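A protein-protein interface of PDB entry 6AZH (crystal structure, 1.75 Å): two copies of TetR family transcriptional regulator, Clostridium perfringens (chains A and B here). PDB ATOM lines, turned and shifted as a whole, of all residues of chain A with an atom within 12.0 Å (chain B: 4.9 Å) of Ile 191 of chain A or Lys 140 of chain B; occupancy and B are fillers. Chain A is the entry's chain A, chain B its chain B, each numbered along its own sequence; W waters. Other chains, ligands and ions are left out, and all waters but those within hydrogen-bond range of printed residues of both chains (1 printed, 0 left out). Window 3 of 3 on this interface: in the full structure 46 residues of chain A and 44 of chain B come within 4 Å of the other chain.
N of Ile 191 of chain A is in hydrogen-bond range of O of Gln 141 of chain B.
The backbone carbonyl oxygen (O) of Ile 189 of chain A lies within hydrogen-bond range of the backbone NH (N) of Arg 143 of chain B (2.7 Å).
NH2 of Arg 143 of chain B is in hydrogen-bond range of O of Gly 188 of chain A (2.9 Å).
The side-chain amide oxygen of Asn 184 of chain A is in hydrogen-bond range of the guanidinium group of Arg 143 of chain B, 2.7 Å away.
The backbone carbonyl oxygen (O) of Ala 136 of chain B lies within hydrogen-bond range of the backbone NH (N) of Gln 141 of chain B, 2.9 Å away.
N of Ile 142 of chain B lies within hydrogen-bond range of O of Ala 136 of chain B.
The backbone carbonyl oxygen (O) of Ile 183 of chain A is in hydrogen-bond range of the backbone NH (N) of Gly 188 of chain A.
Among the printed residues, pairs that only touch across the chains: Ile 183 of chain A with Arg 143 of chain B (3.5 Å), Ile 189 of chain A with Ile 142 of chain B (3.1 Å), Val 190 of chain A with Gln 141 of chain B (3.9 Å), Ile 191 of chain A with Lys 140 of chain B (3.5 Å), Ile 191 of chain A with Ile 142 of chain B (3.7 Å) and Ile 191 of chain A with Arg 143 of chain B (3.6 Å).
Printed residues of chain B within 4 Å of Ile 189 of chain A: Ile 142 (3.1 Å) and Arg 143 (2.7 Å).
Of the printed residues of chain B, Val 190 of chain A touches Gln 141 (3.9 Å).
Ile 191 of chain A touches four residues of chain B.
Ala 136 of chain B touches none of the printed residues of chain A.
No residue of chain A comes within 4 Å of Ser 138 of chain B.
No residue of chain A comes within 4 Å of Lys 139 of chain B.
Gln 141 of chain B touches just these residues of chain A: Val 190 and Ile 191.
Ile 142 of chain B touches two residues of chain A.
Of the printed residues of chain A, Arg 143 of chain B touches Ile 183, Asn 184, Gly 188, Ile 189 and Ile 191.
Of the 8 printed residues of chain B, 4 touch a printed residue of chain A.
Hydrophobic or aromatic side chains of chain B within 4 Å of the printed part of chain A: Ile 142.
Along chain A the printed residues that touch a printed residue of chain B span positions 183 to 191.
Among the printed residues, 10 pairs touch across the chains.
No position is printed for both chains.
Water W1 lies within hydrogen-bond range of the side-chain amide oxygen (OD1) of Asn 184 of chain A (2.6 Å) and the guanidinium group (NH1) of Arg 143 of chain B (2.9 Å).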
ATOM      1  N   ILE A 183     -12.600  25.831  18.707  1.00  0.00           N
ATOM      2  CA  ILE A 183     -12.064  25.123  17.545  1.00  0.00           C
ATOM      3  C   ILE A 183     -10.692  24.541  17.857  1.00  0.00           C
ATOM      4  O   ILE A 183     -10.421  23.374  17.555  1.00  0.00           O
ATOM      5  CB  ILE A 183     -12.032  26.053  16.320  1.00  0.00           C
ATOM      6  CG1 ILE A 183     -13.458  26.367  15.862  1.00  0.00           C
ATOM      7  CG2 ILE A 183     -11.279  25.387  15.180  1.00  0.00           C
ATOM      8  CD1 ILE A 183     -13.552  27.554  14.911  1.00  0.00           C
ATOM      9  N   ASN A 184      -9.812  25.321  18.503  1.00  0.00           N
ATOM     10  CA  ASN A 184      -8.485  24.800  18.817  1.00  0.00           C
ATOM     11  C   ASN A 184      -8.575  23.520  19.639  1.00  0.00           C
ATOM     12  O   ASN A 184      -7.877  22.540  19.358  1.00  0.00           O
ATOM     13  CB  ASN A 184      -7.667  25.846  19.570  1.00  0.00           C
ATOM     14  CG  ASN A 184      -7.303  27.043  18.711  1.00  0.00           C
ATOM     15  OD1 ASN A 184      -7.509  27.044  17.493  1.00  0.00           O
ATOM     16  ND2 ASN A 184      -6.758  28.077  19.348  1.00  0.00           N
ATOM     17  N   LEU A 186     -11.328  21.405  20.147  1.00  0.00           N
ATOM     18  CA  LEU A 186     -12.061  20.281  19.564  1.00  0.00           C
ATOM     19  C   LEU A 186     -11.389  19.761  18.291  1.00  0.00           C
ATOM     20  O   LEU A 186     -11.218  18.546  18.120  1.00  0.00           O
ATOM     21  CB  LEU A 186     -13.520  20.693  19.288  1.00  0.00           C
ATOM     22  CG  LEU A 186     -14.345  21.026  20.543  1.00  0.00           C
ATOM     23  CD1 LEU A 186     -15.800  21.369  20.186  1.00  0.00           C
ATOM     24  CD2 LEU A 186     -14.305  19.869  21.502  1.00  0.00           C
ATOM     25  N   ASP A 187     -10.998  20.663  17.388  1.00  0.00           N
ATOM     26  CA  ASP A 187     -10.466  20.270  16.079  1.00  0.00           C
ATOM     27  C   ASP A 187      -8.943  20.205  16.029  1.00  0.00           C
ATOM     28  O   ASP A 187      -8.393  19.695  15.052  1.00  0.00           O
ATOM     29  CB  ASP A 187     -10.945  21.246  14.997  1.00  0.00           C
ATOM     30  CG  ASP A 187     -12.457  21.241  14.833  1.00  0.00           C
ATOM     31  OD1 ASP A 187     -13.022  20.147  14.688  1.00  0.00           O
ATOM     32  OD2 ASP A 187     -13.074  22.329  14.878  1.00  0.00           O
ATOM     33  N   GLY A 188      -8.249  20.710  17.036  1.00  0.00           N
ATOM     34  CA  GLY A 188      -6.805  20.787  16.946  1.00  0.00           C
ATOM     35  C   GLY A 188      -6.398  21.924  16.037  1.00  0.00           C
ATOM     36  O   GLY A 188      -7.222  22.690  15.546  1.00  0.00           O
ATOM     37  N   ILE A 189      -5.087  22.041  15.813  1.00  0.00           N
ATOM     38  CA  ILE A 189      -4.561  23.103  14.964  1.00  0.00           C
ATOM     39  C   ILE A 189      -4.047  22.604  13.623  1.00  0.00           C
ATOM     40  O   ILE A 189      -3.810  23.430  12.729  1.00  0.00           O
ATOM     41  CB  ILE A 189      -3.455  23.907  15.683  1.00  0.00           C
ATOM     42  CG1 ILE A 189      -2.294  22.992  16.065  1.00  0.00           C
ATOM     43  CG2 ILE A 189      -4.058  24.622  16.897  1.00  0.00           C
ATOM     44  CD1 ILE A 189      -1.112  23.761  16.681  1.00  0.00           C
ATOM     45  N   VAL A 190      -3.893  21.293  13.441  1.00  0.00           N
ATOM     46  CA  VAL A 190      -3.334  20.780  12.197  1.00  0.00           C
ATOM     47  C   VAL A 190      -4.304  21.025  11.048  1.00  0.00           C
ATOM     48  O   VAL A 190      -5.527  20.936  11.203  1.00  0.00           O
ATOM     49  CB  VAL A 190      -2.986  19.289  12.360  1.00  0.00           C
ATOM     50  CG1 VAL A 190      -3.024  18.553  11.037  1.00  0.00           C
ATOM     51  CG2 VAL A 190      -1.609  19.147  12.999  1.00  0.00           C
ATOM     52  N   ILE A 191      -3.755  21.389   9.889  1.00  0.00           N
ATOM     53  CA  ILE A 191      -4.566  21.534   8.688  1.00  0.00           C
ATOM     54  C   ILE A 191      -5.195  20.184   8.343  1.00  0.00           C
ATOM     55  O   ILE A 191      -4.534  19.138   8.377  1.00  0.00           O
ATOM     56  CB  ILE A 191      -3.695  22.125   7.563  1.00  0.00           C
ATOM     57  CG1 ILE A 191      -4.476  23.156   6.752  1.00  0.00           C
ATOM     58  CG2 ILE A 191      -3.050  21.056   6.689  1.00  0.00           C
ATOM     59  CD1 ILE A 191      -4.745  24.421   7.525  1.00  0.00           C
ATOM     60  N   LYS A 192      -6.496  20.187   8.074  1.00  0.00           N
ATOM     61  CA  LYS A 192      -7.200  18.917   7.846  1.00  0.00           C
ATOM     62  C   LYS A 192      -8.023  18.896   6.551  1.00  0.00           C
ATOM     63  O   LYS A 192      -8.312  19.939   5.962  1.00  0.00           O
ATOM     64  CB  LYS A 192      -8.108  18.593   9.039  1.00  0.00           C
ATOM     65  CG  LYS A 192      -7.363  18.410  10.356  1.00  0.00           C
ATOM     66  CD  LYS A 192      -7.998  17.334  11.234  1.00  0.00           C
ATOM     67  CE  LYS A 192      -8.646  17.938  12.474  1.00  0.00           C
ATOM     68  NZ  LYS A 192      -8.472  17.072  13.685  1.00  0.00           N
ATOM     69  N   ALA B 136       4.603  27.958  10.658  1.00  0.00           N
ATOM     70  CA  ALA B 136       3.687  26.857  10.384  1.00  0.00           C
ATOM     71  C   ALA B 136       2.464  27.327   9.603  1.00  0.00           C
ATOM     72  O   ALA B 136       1.943  26.587   8.762  1.00  0.00           O
ATOM     73  CB  ALA B 136       3.271  26.176  11.691  1.00  0.00           C
ATOM     74  N   ILE B 137       1.989  28.548   9.862  1.00  0.00           N
ATOM     75  CA  ILE B 137       0.822  29.047   9.140  1.00  0.00           C
ATOM     76  C   ILE B 137       1.193  29.393   7.701  1.00  0.00           C
ATOM     77  O   ILE B 137       0.442  29.098   6.764  1.00  0.00           O
ATOM     78  CB  ILE B 137       0.205  30.247   9.880  1.00  0.00           C
ATOM     79  CG1 ILE B 137      -0.531  29.761  11.129  1.00  0.00           C
ATOM     80  CG2 ILE B 137      -0.771  30.986   8.990  1.00  0.00           C
ATOM     81  CD1 ILE B 137      -1.261  30.855  11.844  1.00  0.00           C
ATOM     82  N   SER B 138       2.360  30.009   7.503  1.00  0.00           N
ATOM     83  CA  SER B 138       2.798  30.325   6.147  1.00  0.00           C
ATOM     84  C   SER B 138       2.989  29.057   5.316  1.00  0.00           C
ATOM     85  O   SER B 138       2.612  29.021   4.140  1.00  0.00           O
ATOM     86  CB  SER B 138       4.085  31.147   6.192  1.00  0.00           C
ATOM     87  OG  SER B 138       5.143  30.381   6.742  1.00  0.00           O
ATOM     88  N   LYS B 139       3.549  27.999   5.915  1.00  0.00           N
ATOM     89  CA  LYS B 139       3.711  26.708   5.248  1.00  0.00           C
ATOM     90  C   LYS B 139       2.416  25.906   5.154  1.00  0.00           C
ATOM     91  O   LYS B 139       2.450  24.762   4.675  1.00  0.00           O
ATOM     92  CB  LYS B 139       4.768  25.870   5.972  1.00  0.00           C
ATOM     93  CG  LYS B 139       6.199  26.242   5.639  1.00  0.00           C
ATOM     94  CD  LYS B 139       6.751  25.312   4.568  1.00  0.00           C
ATOM     95  CE  LYS B 139       8.239  25.513   4.364  1.00  0.00           C
ATOM     96  NZ  LYS B 139       8.963  25.590   5.672  1.00  0.00           N
ATOM     97  N   LYS B 140       1.288  26.455   5.615  1.00  0.00           N
ATOM     98  CA  LYS B 140      -0.010  25.774   5.556  1.00  0.00           C
ATOM     99  C   LYS B 140       0.010  24.438   6.300  1.00  0.00           C
ATOM    100  O   LYS B 140      -0.664  23.481   5.908  1.00  0.00           O
ATOM    101  CB  LYS B 140      -0.464  25.563   4.105  1.00  0.00           C
ATOM    102  CG  LYS B 140      -0.367  26.801   3.228  1.00  0.00           C
ATOM    103  CD  LYS B 140      -1.549  27.735   3.449  1.00  0.00           C
ATOM    104  CE  LYS B 140      -1.756  28.677   2.267  1.00  0.00           C
ATOM    105  NZ  LYS B 140      -0.621  29.632   2.095  1.00  0.00           N
ATOM    106  N   GLN B 141       0.785  24.351   7.381  1.00  0.00           N
ATOM    107  CA  GLN B 141       0.837  23.125   8.159  1.00  0.00           C
ATOM    108  C   GLN B 141      -0.111  23.141   9.353  1.00  0.00           C
ATOM    109  O   GLN B 141      -0.487  22.072   9.843  1.00  0.00           O
ATOM    110  CB  GLN B 141       2.270  22.867   8.632  1.00  0.00           C
ATOM    111  CG  GLN B 141       3.150  22.237   7.556  1.00  0.00           C
ATOM    112  CD  GLN B 141       4.613  22.530   7.767  1.00  0.00           C
ATOM    113  OE1 GLN B 141       5.049  22.772   8.892  1.00  0.00           O
ATOM    114  NE2 GLN B 141       5.393  22.499   6.680  1.00  0.00           N
ATOM    115  N   ILE B 142      -0.503  24.322   9.823  1.00  0.00           N
ATOM    116  CA  ILE B 142      -1.542  24.472  10.831  1.00  0.00           C
ATOM    117  C   ILE B 142      -2.533  25.517  10.338  1.00  0.00           C
ATOM    118  O   ILE B 142      -2.238  26.312   9.445  1.00  0.00           O
ATOM    119  CB  ILE B 142      -0.991  24.885  12.211  1.00  0.00           C
ATOM    120  CG1 ILE B 142      -0.558  26.351  12.183  1.00  0.00           C
ATOM    121  CG2 ILE B 142       0.160  23.988  12.649  1.00  0.00           C
ATOM    122  CD1 ILE B 142      -0.235  26.896  13.576  1.00  0.00           C
ATOM    123  N   ARG B 143      -3.718  25.517  10.951  1.00  0.00           N
ATOM    124  CA  ARG B 143      -4.778  26.437  10.550  1.00  0.00           C
ATOM    125  C   ARG B 143      -4.378  27.890  10.772  1.00  0.00           C
ATOM    126  O   ARG B 143      -3.609  28.220  11.681  1.00  0.00           O
ATOM    127  CB  ARG B 143      -6.057  26.176  11.346  1.00  0.00           C
ATOM    128  CG  ARG B 143      -6.926  25.057  10.860  1.00  0.00           C
ATOM    129  CD  ARG B 143      -8.218  25.028  11.665  1.00  0.00           C
ATOM    130  NE  ARG B 143      -7.961  24.832  13.090  1.00  0.00           N
ATOM    131  CZ  ARG B 143      -7.979  25.800  14.008  1.00  0.00           C
ATOM    132  NH1 ARG B 143      -8.233  27.062  13.662  1.00  0.00           N
ATOM    133  NH2 ARG B 143      -7.724  25.502  15.277  1.00  0.00           N
HETATM  134  O   HOH W   1      -8.642  28.828  15.922  1.00  0.00           O
